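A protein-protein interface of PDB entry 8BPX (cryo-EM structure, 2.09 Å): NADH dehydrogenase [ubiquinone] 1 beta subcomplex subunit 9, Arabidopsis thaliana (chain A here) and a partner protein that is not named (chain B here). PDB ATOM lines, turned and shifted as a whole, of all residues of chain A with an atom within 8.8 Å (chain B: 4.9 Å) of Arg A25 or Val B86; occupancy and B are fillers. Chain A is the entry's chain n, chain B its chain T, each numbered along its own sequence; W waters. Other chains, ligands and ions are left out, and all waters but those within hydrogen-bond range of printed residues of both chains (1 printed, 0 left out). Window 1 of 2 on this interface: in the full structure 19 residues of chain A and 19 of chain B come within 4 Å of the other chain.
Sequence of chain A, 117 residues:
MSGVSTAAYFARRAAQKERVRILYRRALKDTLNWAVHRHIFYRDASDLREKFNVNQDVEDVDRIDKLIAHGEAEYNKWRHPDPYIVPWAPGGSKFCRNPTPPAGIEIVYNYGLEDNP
The side-chain hydroxyl (OH) of Tyr A24 lies within hydrogen-bond range of the side-chain carboxylate (OE2) of Glu B84 (2.7 Å). The side-chain carboxylate (OE2) of Glu B90 is in salt-bridge range of the guanidinium group (NH2) of Arg A25 (3.1 Å). O of Ile B97 is in hydrogen-bond range of NH2 of Arg A25. OD1 of Asp B99 lies within salt-bridge range of NE of Arg A25, 3.1 Å away. The guanidinium group (NH1) of Arg A26 is in salt-bridge range of the side-chain carboxylate (OD2) of Asp B99, 2.7 Å away.
The side-chain carboxylate (OE2) of Glu B90 is in hydrogen-bond range of the backbone NH (N) of Ile B97 (2.4 Å). The backbone carbonyl oxygen of Arg A25 lies close to the side-chain amino group of Lys A29.
Among the printed residues, merely in contact across the chains: Arg A25 with Ala B102 (3.5 Å), Arg A25 with Val B83 (3.5 Å), Phe A41 with Met B87 (3.8 Å), Leu A28 with Met B87 (3.8 Å), Ile A22 with Asp B99 (3.8 Å), Leu A32 with Met B87 (3.9 Å), Lys A29 with Met B87 (3.9 Å), Arg A25 with Val B86 (3.9 Å), Tyr A24 with Val B83 (3.9 Å), Arg A21 with Val B83 (3.9 Å) and Leu A28 with Glu B84 (3.998 Å).
Of chain B, only Val B83, Val B86, Glu B90, Ile B97, Asp B99 and Ala B102 come within 4 Å of Arg A25. Of chain A, only Arg A25 (3.9 Å) comes within 4 Å of Val B86. Of the printed residues of chain A, Met B87 touches Leu A28 (3.8 Å), Lys A29 (3.9 Å), Leu A32 (3.9 Å) and Phe A41 (3.8 Å). Printed residues of chain B within 4 Å of Arg A26: Asp B99 (2.7 Å). Leu A48 touches none of the printed residues of chain B. The nearest residue of chain A that does not touch Val B86 is Lys A29 (6.5 Å). The nearest printed residue of chain B that does not touch Leu A28 is Val B83 (5.3 Å).
Of the 21 printed residues of chain A, 9 touch a printed residue of chain B. Hydrophobic or aromatic side chains of chain A that line the printed part of chain B: Ile A22, Tyr A24, Leu A28, Leu A32 and Phe A41. Along chain A the printed residues that touch a printed residue of chain B span positions 21 to 41. Hydrophobic or aromatic side chains of chain B within 4 Å of the printed part of chain A: Val B83, Val B86, Met B87 and Ala B102.
Water W1 lies within hydrogen-bond range of the guanidinium group (NH1) of Arg A25 (2.7 Å), the backbone carbonyl oxygen (O) of Val B83 (2.8 Å) and the backbone NH (N) of Met B87 (3.4 Å).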
ATOM      1  N   GLU A  18      35.957  22.188  -2.302  1.00  0.00           N
ATOM      2  CA  GLU A  18      34.636  22.784  -2.161  1.00  0.00           C
ATOM      3  C   GLU A  18      33.777  22.503  -3.385  1.00  0.00           C
ATOM      4  O   GLU A  18      32.598  22.148  -3.257  1.00  0.00           O
ATOM      5  CB  GLU A  18      34.787  24.288  -1.891  1.00  0.00           C
ATOM      6  CG  GLU A  18      33.552  25.164  -2.095  1.00  0.00           C
ATOM      7  CD  GLU A  18      33.216  25.405  -3.566  1.00  0.00           C
ATOM      8  OE1 GLU A  18      34.075  25.948  -4.293  1.00  0.00           O
ATOM      9  OE2 GLU A  18      32.107  25.038  -3.999  1.00  0.00           O
ATOM     10  N   ARG A  19      34.354  22.654  -4.578  1.00  0.00           N
ATOM     11  CA  ARG A  19      33.609  22.385  -5.800  1.00  0.00           C
ATOM     12  C   ARG A  19      33.141  20.938  -5.842  1.00  0.00           C
ATOM     13  O   ARG A  19      31.977  20.661  -6.143  1.00  0.00           O
ATOM     14  CB  ARG A  19      34.471  22.706  -7.022  1.00  0.00           C
ATOM     15  CG  ARG A  19      34.945  24.150  -7.098  1.00  0.00           C
ATOM     16  CD  ARG A  19      33.889  25.068  -7.669  1.00  0.00           C
ATOM     17  NE  ARG A  19      33.518  24.710  -9.031  1.00  0.00           N
ATOM     18  CZ  ARG A  19      34.256  24.962 -10.102  1.00  0.00           C
ATOM     19  NH1 ARG A  19      35.417  25.585 -10.012  1.00  0.00           N
ATOM     20  NH2 ARG A  19      33.814  24.580 -11.297  1.00  0.00           N
ATOM     21  N   VAL A  20      34.019  19.999  -5.512  1.00  0.00           N
ATOM     22  CA  VAL A  20      33.660  18.562  -5.528  1.00  0.00           C
ATOM     23  C   VAL A  20      32.572  18.269  -4.467  1.00  0.00           C
ATOM     24  O   VAL A  20      31.582  17.703  -4.856  1.00  0.00           O
ATOM     25  CB  VAL A  20      34.872  17.614  -5.470  1.00  0.00           C
ATOM     26  CG1 VAL A  20      34.479  16.148  -5.447  1.00  0.00           C
ATOM     27  CG2 VAL A  20      35.864  17.905  -6.575  1.00  0.00           C
ATOM     28  N   ARG A  21      32.726  18.758  -3.240  1.00  0.00           N
ATOM     29  CA  ARG A  21      31.736  18.546  -2.148  1.00  0.00           C
ATOM     30  C   ARG A  21      30.363  19.139  -2.489  1.00  0.00           C
ATOM     31  O   ARG A  21      29.368  18.546  -2.121  1.00  0.00           O
ATOM     32  CB  ARG A  21      32.310  19.014  -0.812  1.00  0.00           C
ATOM     33  CG  ARG A  21      33.398  18.111  -0.250  1.00  0.00           C
ATOM     34  CD  ARG A  21      33.688  18.428   1.200  1.00  0.00           C
ATOM     35  NE  ARG A  21      33.812  19.854   1.383  1.00  0.00           N
ATOM     36  CZ  ARG A  21      34.942  20.539   1.331  1.00  0.00           C
ATOM     37  NH1 ARG A  21      36.090  19.917   1.151  1.00  0.00           N
ATOM     38  NH2 ARG A  21      34.908  21.847   1.466  1.00  0.00           N
ATOM     39  N   ILE A  22      30.322  20.273  -3.165  1.00  0.00           N
ATOM     40  CA  ILE A  22      29.047  20.869  -3.543  1.00  0.00           C
ATOM     41  C   ILE A  22      28.443  20.145  -4.744  1.00  0.00           C
ATOM     42  O   ILE A  22      27.223  19.925  -4.802  1.00  0.00           O
ATOM     43  CB  ILE A  22      29.237  22.379  -3.792  1.00  0.00           C
ATOM     44  CG1 ILE A  22      29.513  23.078  -2.456  1.00  0.00           C
ATOM     45  CG2 ILE A  22      28.039  22.983  -4.517  1.00  0.00           C
ATOM     46  CD1 ILE A  22      29.445  24.575  -2.500  1.00  0.00           C
ATOM     47  N   LEU A  23      29.285  19.732  -5.683  1.00  0.00           N
ATOM     48  CA  LEU A  23      28.819  18.946  -6.850  1.00  0.00           C
ATOM     49  C   LEU A  23      28.178  17.647  -6.339  1.00  0.00           C
ATOM     50  O   LEU A  23      27.054  17.324  -6.793  1.00  0.00           O
ATOM     51  CB  LEU A  23      29.957  18.651  -7.829  1.00  0.00           C
ATOM     52  CG  LEU A  23      29.618  17.698  -8.976  1.00  0.00           C
ATOM     53  CD1 LEU A  23      28.602  18.305  -9.923  1.00  0.00           C
ATOM     54  CD2 LEU A  23      30.856  17.261  -9.729  1.00  0.00           C
ATOM     55  N   TYR A  24      28.853  16.958  -5.441  1.00  0.00           N
ATOM     56  CA  TYR A  24      28.329  15.698  -4.929  1.00  0.00           C
ATOM     57  C   TYR A  24      27.003  15.904  -4.209  1.00  0.00           C
ATOM     58  O   TYR A  24      26.067  15.117  -4.384  1.00  0.00           O
ATOM     59  CB  TYR A  24      29.343  15.041  -3.998  1.00  0.00           C
ATOM     60  CG  TYR A  24      28.856  13.734  -3.426  1.00  0.00           C
ATOM     61  CD1 TYR A  24      28.335  12.747  -4.249  1.00  0.00           C
ATOM     62  CD2 TYR A  24      28.883  13.500  -2.061  1.00  0.00           C
ATOM     63  CE1 TYR A  24      27.877  11.560  -3.733  1.00  0.00           C
ATOM     64  CE2 TYR A  24      28.427  12.310  -1.535  1.00  0.00           C
ATOM     65  CZ  TYR A  24      27.924  11.345  -2.376  1.00  0.00           C
ATOM     66  OH  TYR A  24      27.465  10.160  -1.861  1.00  0.00           O
ATOM     67  N   ARG A  25      26.884  16.937  -3.390  1.00  0.00           N
ATOM     68  CA  ARG A  25      25.639  17.238  -2.678  1.00  0.00           C
ATOM     69  C   ARG A  25      24.447  17.435  -3.652  1.00  0.00           C
ATOM     70  O   ARG A  25      23.379  16.927  -3.365  1.00  0.00           O
ATOM     71  CB  ARG A  25      25.840  18.433  -1.736  1.00  0.00           C
ATOM     72  CG  ARG A  25      24.579  19.212  -1.410  1.00  0.00           C
ATOM     73  CD  ARG A  25      24.723  19.991  -0.125  1.00  0.00           C
ATOM     74  NE  ARG A  25      23.534  20.741   0.211  1.00  0.00           N
ATOM     75  CZ  ARG A  25      22.683  20.416   1.172  1.00  0.00           C
ATOM     76  NH1 ARG A  25      22.881  19.343   1.913  1.00  0.00           N
ATOM     77  NH2 ARG A  25      21.634  21.172   1.390  1.00  0.00           N
ATOM     78  N   ARG A  26      24.666  18.152  -4.729  1.00  0.00           N
ATOM     79  CA  ARG A  26      23.608  18.493  -5.686  1.00  0.00           C
ATOM     80  C   ARG A  26      23.252  17.245  -6.505  1.00  0.00           C
ATOM     81  O   ARG A  26      22.094  17.070  -6.698  1.00  0.00           O
ATOM     82  CB  ARG A  26      24.004  19.746  -6.483  1.00  0.00           C
ATOM     83  CG  ARG A  26      24.199  21.029  -5.697  1.00  0.00           C
ATOM     84  CD  ARG A  26      23.963  22.193  -6.639  1.00  0.00           C
ATOM     85  NE  ARG A  26      25.100  22.792  -7.304  1.00  0.00           N
ATOM     86  CZ  ARG A  26      25.699  23.932  -6.951  1.00  0.00           C
ATOM     87  NH1 ARG A  26      25.266  24.644  -5.929  1.00  0.00           N
ATOM     88  NH2 ARG A  26      26.740  24.361  -7.633  1.00  0.00           N
ATOM     89  N   ALA A  27      24.239  16.451  -6.897  1.00  0.00           N
ATOM     90  CA  ALA A  27      24.017  15.189  -7.654  1.00  0.00           C
ATOM     91  C   ALA A  27      23.195  14.241  -6.788  1.00  0.00           C
ATOM     92  O   ALA A  27      22.191  13.752  -7.289  1.00  0.00           O
ATOM     93  CB  ALA A  27      25.330  14.580  -8.151  1.00  0.00           C
ATOM     94  N   LEU A  28      23.492  14.185  -5.493  1.00  0.00           N
ATOM     95  CA  LEU A  28      22.804  13.269  -4.562  1.00  0.00           C
ATOM     96  C   LEU A  28      21.354  13.693  -4.378  1.00  0.00           C
ATOM     97  O   LEU A  28      20.500  12.835  -4.452  1.00  0.00           O
ATOM     98  CB  LEU A  28      23.618  13.186  -3.270  1.00  0.00           C
ATOM     99  CG  LEU A  28      23.312  12.072  -2.283  1.00  0.00           C
ATOM    100  CD1 LEU A  28      23.393  10.715  -2.950  1.00  0.00           C
ATOM    101  CD2 LEU A  28      24.287  12.160  -1.125  1.00  0.00           C
ATOM    102  N   LYS A  29      21.109  14.986  -4.286  1.00  0.00           N
ATOM    103  CA  LYS A  29      19.746  15.513  -4.061  1.00  0.00           C
ATOM    104  C   LYS A  29      18.896  15.280  -5.316  1.00  0.00           C
ATOM    105  O   LYS A  29      17.743  14.893  -5.172  1.00  0.00           O
ATOM    106  CB  LYS A  29      19.851  16.919  -3.447  1.00  0.00           C
ATOM    107  CG  LYS A  29      19.697  16.891  -1.933  1.00  0.00           C
ATOM    108  CD  LYS A  29      19.540  18.222  -1.261  1.00  0.00           C
ATOM    109  CE  LYS A  29      20.877  18.879  -1.024  1.00  0.00           C
ATOM    110  NZ  LYS A  29      21.896  17.880  -0.624  1.00  0.00           N
ATOM    111  N   ASP A  30      19.529  15.359  -6.473  1.00  0.00           N
ATOM    112  CA  ASP A  30      18.856  15.127  -7.745  1.00  0.00           C
ATOM    113  C   ASP A  30      18.592  13.635  -7.977  1.00  0.00           C
ATOM    114  O   ASP A  30      17.668  13.356  -8.666  1.00  0.00           O
ATOM    115  CB  ASP A  30      19.648  15.772  -8.869  1.00  0.00           C
ATOM    116  CG  ASP A  30      18.777  16.234 -10.010  1.00  0.00           C
ATOM    117  OD1 ASP A  30      17.986  17.157  -9.793  1.00  0.00           O
ATOM    118  OD2 ASP A  30      18.900  15.651 -11.098  1.00  0.00           O
ATOM    119  N   THR A  31      19.442  12.780  -7.461  1.00  0.00           N
ATOM    120  CA  THR A  31      19.246  11.320  -7.557  1.00  0.00           C
ATOM    121  C   THR A  31      17.896  10.996  -6.903  1.00  0.00           C
ATOM    122  O   THR A  31      17.154  10.280  -7.535  1.00  0.00           O
ATOM    123  CB  THR A  31      20.524  10.589  -7.100  1.00  0.00           C
ATOM    124  OG1 THR A  31      21.483  10.544  -8.149  1.00  0.00           O
ATOM    125  CG2 THR A  31      20.259   9.202  -6.571  1.00  0.00           C
ATOM    126  N   LEU A  32      17.556  11.669  -5.814  1.00  0.00           N
ATOM    127  CA  LEU A  32      16.267  11.502  -5.126  1.00  0.00           C
ATOM    128  C   LEU A  32      15.102  12.039  -5.963  1.00  0.00           C
ATOM    129  O   LEU A  32      14.090  11.373  -5.937  1.00  0.00           O
ATOM    130  CB  LEU A  32      16.376  12.050  -3.705  1.00  0.00           C
ATOM    131  CG  LEU A  32      15.192  11.818  -2.769  1.00  0.00           C
ATOM    132  CD1 LEU A  32      14.832  10.348  -2.670  1.00  0.00           C
ATOM    133  CD2 LEU A  32      15.506  12.375  -1.399  1.00  0.00           C
ATOM    134  N   ASN A  33      15.253  13.136  -6.697  1.00  0.00           N
ATOM    135  CA  ASN A  33      14.211  13.659  -7.614  1.00  0.00           C
ATOM    136  C   ASN A  33      13.849  12.658  -8.716  1.00  0.00           C
ATOM    137  O   ASN A  33      12.699  12.593  -9.064  1.00  0.00           O
ATOM    138  CB  ASN A  33      14.579  15.039  -8.200  1.00  0.00           C
ATOM    139  CG  ASN A  33      14.793  16.124  -7.173  1.00  0.00           C
ATOM    140  OD1 ASN A  33      13.997  16.267  -6.266  1.00  0.00           O
ATOM    141  ND2 ASN A  33      15.846  16.905  -7.328  1.00  0.00           N
ATOM    142  N   PHE A  41      16.438   4.951  -4.515  1.00  0.00           N
ATOM    143  CA  PHE A  41      17.443   5.989  -4.131  1.00  0.00           C
ATOM    144  C   PHE A  41      18.687   5.301  -3.550  1.00  0.00           C
ATOM    145  O   PHE A  41      19.767   5.672  -3.921  1.00  0.00           O
ATOM    146  CB  PHE A  41      16.888   7.105  -3.232  1.00  0.00           C
ATOM    147  CG  PHE A  41      17.883   8.074  -2.649  1.00  0.00           C
ATOM    148  CD1 PHE A  41      18.549   8.982  -3.454  1.00  0.00           C
ATOM    149  CD2 PHE A  41      18.123   8.107  -1.284  1.00  0.00           C
ATOM    150  CE1 PHE A  41      19.460   9.875  -2.911  1.00  0.00           C
ATOM    151  CE2 PHE A  41      19.027   9.003  -0.744  1.00  0.00           C
ATOM    152  CZ  PHE A  41      19.688   9.891  -1.557  1.00  0.00           C
ATOM    153  N   LEU A  48      26.321   6.673  -7.596  1.00  0.00           N
ATOM    154  CA  LEU A  48      26.909   8.028  -7.746  1.00  0.00           C
ATOM    155  C   LEU A  48      28.166   8.160  -6.875  1.00  0.00           C
ATOM    156  O   LEU A  48      29.273   8.723  -7.347  1.00  0.00           O
ATOM    157  CB  LEU A  48      25.828   9.056  -7.419  1.00  0.00           C
ATOM    158  CG  LEU A  48      26.260  10.513  -7.376  1.00  0.00           C
ATOM    159  CD1 LEU A  48      26.295  11.107  -8.770  1.00  0.00           C
ATOM    160  CD2 LEU A  48      25.330  11.291  -6.470  1.00  0.00           C
ATOM    161  N   PHE A  52      32.271   9.108  -7.869  1.00  0.00           N
ATOM    162  CA  PHE A  52      33.285   9.990  -7.216  1.00  0.00           C
ATOM    163  C   PHE A  52      34.441   9.150  -6.635  1.00  0.00           C
ATOM    164  O   PHE A  52      35.586   9.538  -6.699  1.00  0.00           O
ATOM    165  CB  PHE A  52      32.664  10.920  -6.180  1.00  0.00           C
ATOM    166  CG  PHE A  52      31.740  11.995  -6.699  1.00  0.00           C
ATOM    167  CD1 PHE A  52      30.488  11.680  -7.202  1.00  0.00           C
ATOM    168  CD2 PHE A  52      32.105  13.329  -6.655  1.00  0.00           C
ATOM    169  CE1 PHE A  52      29.632  12.665  -7.659  1.00  0.00           C
ATOM    170  CE2 PHE A  52      31.251  14.316  -7.115  1.00  0.00           C
ATOM    171  CZ  PHE A  52      30.016  13.983  -7.617  1.00  0.00           C
ATOM    172  N   GLU A  72      30.371  19.187 -13.431  1.00  0.00           N
ATOM    173  CA  GLU A  72      29.376  20.256 -13.426  1.00  0.00           C
ATOM    174  C   GLU A  72      28.561  20.260 -14.710  1.00  0.00           C
ATOM    175  O   GLU A  72      27.342  20.453 -14.676  1.00  0.00           O
ATOM    176  CB  GLU A  72      30.029  21.624 -13.229  1.00  0.00           C
ATOM    177  CG  GLU A  72      31.137  21.679 -12.218  1.00  0.00           C
ATOM    178  CD  GLU A  72      30.658  22.101 -10.858  1.00  0.00           C
ATOM    179  OE1 GLU A  72      29.820  21.382 -10.273  1.00  0.00           O
ATOM    180  OE2 GLU A  72      31.119  23.158 -10.376  1.00  0.00           O
ATOM    181  N   TYR A  75      26.024  17.328 -14.386  1.00  0.00           N
ATOM    182  CA  TYR A  75      24.921  17.774 -13.521  1.00  0.00           C
ATOM    183  C   TYR A  75      23.995  18.699 -14.290  1.00  0.00           C
ATOM    184  O   TYR A  75      22.809  18.388 -14.409  1.00  0.00           O
ATOM    185  CB  TYR A  75      25.359  18.472 -12.234  1.00  0.00           C
ATOM    186  CG  TYR A  75      24.260  19.047 -11.386  1.00  0.00           C
ATOM    187  CD1 TYR A  75      23.482  18.232 -10.579  1.00  0.00           C
ATOM    188  CD2 TYR A  75      24.008  20.406 -11.379  1.00  0.00           C
ATOM    189  CE1 TYR A  75      22.465  18.751  -9.804  1.00  0.00           C
ATOM    190  CE2 TYR A  75      23.000  20.943 -10.604  1.00  0.00           C
ATOM    191  CZ  TYR A  75      22.230  20.113  -9.812  1.00  0.00           C
ATOM    192  OH  TYR A  75      21.237  20.643  -9.052  1.00  0.00           O
ATOM    193  N   THR B  82      30.694  13.215   4.981  1.00  0.00           N
ATOM    194  CA  THR B  82      30.181  14.387   5.719  1.00  0.00           C
ATOM    195  C   THR B  82      28.990  14.927   4.922  1.00  0.00           C
ATOM    196  O   THR B  82      27.994  15.205   5.521  1.00  0.00           O
ATOM    197  CB  THR B  82      31.308  15.411   5.995  1.00  0.00           C
ATOM    198  OG1 THR B  82      32.281  14.718   6.772  1.00  0.00           O
ATOM    199  CG2 THR B  82      30.824  16.669   6.674  1.00  0.00           C
ATOM    200  N   VAL B  83      29.128  15.000   3.613  1.00  0.00           N
ATOM    201  CA  VAL B  83      28.030  15.484   2.778  1.00  0.00           C
ATOM    202  C   VAL B  83      26.797  14.606   2.957  1.00  0.00           C
ATOM    203  O   VAL B  83      25.669  15.104   3.074  1.00  0.00           O
ATOM    204  CB  VAL B  83      28.472  15.551   1.303  1.00  0.00           C
ATOM    205  CG1 VAL B  83      27.366  16.116   0.449  1.00  0.00           C
ATOM    206  CG2 VAL B  83      29.723  16.390   1.161  1.00  0.00           C
ATOM    207  N   GLU B  84      26.993  13.286   2.984  1.00  0.00           N
ATOM    208  CA  GLU B  84      25.871  12.382   3.224  1.00  0.00           C
ATOM    209  C   GLU B  84      25.234  12.618   4.591  1.00  0.00           C
ATOM    210  O   GLU B  84      24.005  12.628   4.716  1.00  0.00           O
ATOM    211  CB  GLU B  84      26.325  10.928   3.087  1.00  0.00           C
ATOM    212  CG  GLU B  84      26.636  10.513   1.659  1.00  0.00           C
ATOM    213  CD  GLU B  84      27.672   9.415   1.586  1.00  0.00           C
ATOM    214  OE1 GLU B  84      27.918   8.761   2.618  1.00  0.00           O
ATOM    215  OE2 GLU B  84      28.235   9.197   0.496  1.00  0.00           O
ATOM    216  N   ILE B  85      26.053  12.807   5.629  1.00  0.00           N
ATOM    217  CA  ILE B  85      25.516  13.022   6.973  1.00  0.00           C
ATOM    218  C   ILE B  85      24.747  14.339   7.040  1.00  0.00           C
ATOM    219  O   ILE B  85      23.703  14.434   7.699  1.00  0.00           O
ATOM    220  CB  ILE B  85      26.643  12.963   8.023  1.00  0.00           C
ATOM    221  CG1 ILE B  85      27.028  11.515   8.329  1.00  0.00           C
ATOM    222  CG2 ILE B  85      26.228  13.658   9.311  1.00  0.00           C
ATOM    223  CD1 ILE B  85      28.518  11.282   8.453  1.00  0.00           C
ATOM    224  N   VAL B  86      25.244  15.373   6.360  1.00  0.00           N
ATOM    225  CA  VAL B  86      24.533  16.647   6.331  1.00  0.00           C
ATOM    226  C   VAL B  86      23.196  16.496   5.615  1.00  0.00           C
ATOM    227  O   VAL B  86      22.180  17.038   6.059  1.00  0.00           O
ATOM    228  CB  VAL B  86      25.411  17.740   5.696  1.00  0.00           C
ATOM    229  CG1 VAL B  86      24.598  18.999   5.425  1.00  0.00           C
ATOM    230  CG2 VAL B  86      26.589  18.057   6.599  1.00  0.00           C
ATOM    231  N   MET B  87      23.157  15.763   4.485  1.00  0.00           N
ATOM    232  CA  MET B  87      21.876  15.454   3.786  1.00  0.00           C
ATOM    233  C   MET B  87      20.929  14.679   4.728  1.00  0.00           C
ATOM    234  O   MET B  87      19.767  14.978   4.724  1.00  0.00           O
ATOM    235  CB  MET B  87      22.061  14.713   2.453  1.00  0.00           C
ATOM    236  CG  MET B  87      20.753  14.413   1.717  1.00  0.00           C
ATOM    237  SD  MET B  87      20.840  13.700   0.039  1.00  0.00           S
ATOM    238  CE  MET B  87      19.108  13.385  -0.295  1.00  0.00           C
ATOM    239  N   ALA B  88      21.463  13.780   5.541  1.00  0.00           N
ATOM    240  CA  ALA B  88      20.613  13.032   6.465  1.00  0.00           C
ATOM    241  C   ALA B  88      20.043  13.936   7.555  1.00  0.00           C
ATOM    242  O   ALA B  88      18.880  13.793   7.939  1.00  0.00           O
ATOM    243  CB  ALA B  88      21.392  11.875   7.078  1.00  0.00           C
ATOM    244  N   ILE B  89      20.849  14.870   8.064  1.00  0.00           N
ATOM    245  CA  ILE B  89      20.353  15.847   9.035  1.00  0.00           C
ATOM    246  C   ILE B  89      19.274  16.722   8.401  1.00  0.00           C
ATOM    247  O   ILE B  89      18.243  17.029   9.022  1.00  0.00           O
ATOM    248  CB  ILE B  89      21.522  16.686   9.584  1.00  0.00           C
ATOM    249  CG1 ILE B  89      22.375  15.855  10.542  1.00  0.00           C
ATOM    250  CG2 ILE B  89      21.019  17.945  10.278  1.00  0.00           C
ATOM    251  CD1 ILE B  89      23.802  16.352  10.685  1.00  0.00           C
ATOM    252  N   GLU B  90      19.506  17.138   7.153  1.00  0.00           N
ATOM    253  CA  GLU B  90      18.522  17.894   6.387  1.00  0.00           C
ATOM    254  C   GLU B  90      17.185  17.168   6.345  1.00  0.00           C
ATOM    255  O   GLU B  90      16.134  17.757   6.618  1.00  0.00           O
ATOM    256  CB  GLU B  90      19.039  18.110   4.962  1.00  0.00           C
ATOM    257  CG  GLU B  90      20.026  19.240   4.776  1.00  0.00           C
ATOM    258  CD  GLU B  90      19.340  20.571   4.617  1.00  0.00           C
ATOM    259  OE1 GLU B  90      18.733  21.034   5.599  1.00  0.00           O
ATOM    260  OE2 GLU B  90      19.405  21.155   3.516  1.00  0.00           O
ATOM    261  N   ILE B  97      19.140  23.566   3.558  1.00  0.00           N
ATOM    262  CA  ILE B  97      20.324  24.388   3.811  1.00  0.00           C
ATOM    263  C   ILE B  97      20.910  24.836   2.475  1.00  0.00           C
ATOM    264  O   ILE B  97      21.039  24.013   1.558  1.00  0.00           O
ATOM    265  CB  ILE B  97      21.350  23.613   4.630  1.00  0.00           C
ATOM    266  CG1 ILE B  97      20.777  23.278   6.002  1.00  0.00           C
ATOM    267  CG2 ILE B  97      22.627  24.425   4.791  1.00  0.00           C
ATOM    268  CD1 ILE B  97      21.530  22.207   6.744  1.00  0.00           C
ATOM    269  N   ASP B  99      23.706  25.609  -0.260  1.00  0.00           N
ATOM    270  CA  ASP B  99      24.874  24.776  -0.531  1.00  0.00           C
ATOM    271  C   ASP B  99      26.152  25.363   0.056  1.00  0.00           C
ATOM    272  O   ASP B  99      27.041  24.612   0.472  1.00  0.00           O
ATOM    273  CB  ASP B  99      25.032  24.569  -2.036  1.00  0.00           C
ATOM    274  CG  ASP B  99      23.997  23.624  -2.608  1.00  0.00           C
ATOM    275  OD1 ASP B  99      23.246  23.009  -1.825  1.00  0.00           O
ATOM    276  OD2 ASP B  99      23.924  23.502  -3.850  1.00  0.00           O
ATOM    277  N   ALA B 102      25.934  24.421   3.744  1.00  0.00           N
ATOM    278  CA  ALA B 102      26.031  22.984   3.971  1.00  0.00           C
ATOM    279  C   ALA B 102      27.481  22.513   3.922  1.00  0.00           C
ATOM    280  O   ALA B 102      27.884  21.643   4.701  1.00  0.00           O
ATOM    281  CB  ALA B 102      25.181  22.228   2.950  1.00  0.00           C
ATOM    282  N   ILE B 105      29.288  23.047   7.443  1.00  0.00           N
ATOM    283  CA  ILE B 105      29.006  22.078   8.550  1.00  0.00           C
ATOM    284  C   ILE B 105      29.939  20.855   8.456  1.00  0.00           C
ATOM    285  O   ILE B 105      29.738  20.070   7.547  1.00  0.00           O
ATOM    286  CB  ILE B 105      27.516  21.697   8.598  1.00  0.00           C
ATOM    287  CG1 ILE B 105      26.636  22.939   8.728  1.00  0.00           C
ATOM    288  CG2 ILE B 105      27.288  20.706   9.721  1.00  0.00           C
ATOM    289  CD1 ILE B 105      25.244  22.782   8.214  1.00  0.00           C
HETATM  290  O   HOH W   1      24.921  17.696   2.328  1.00  0.00           O
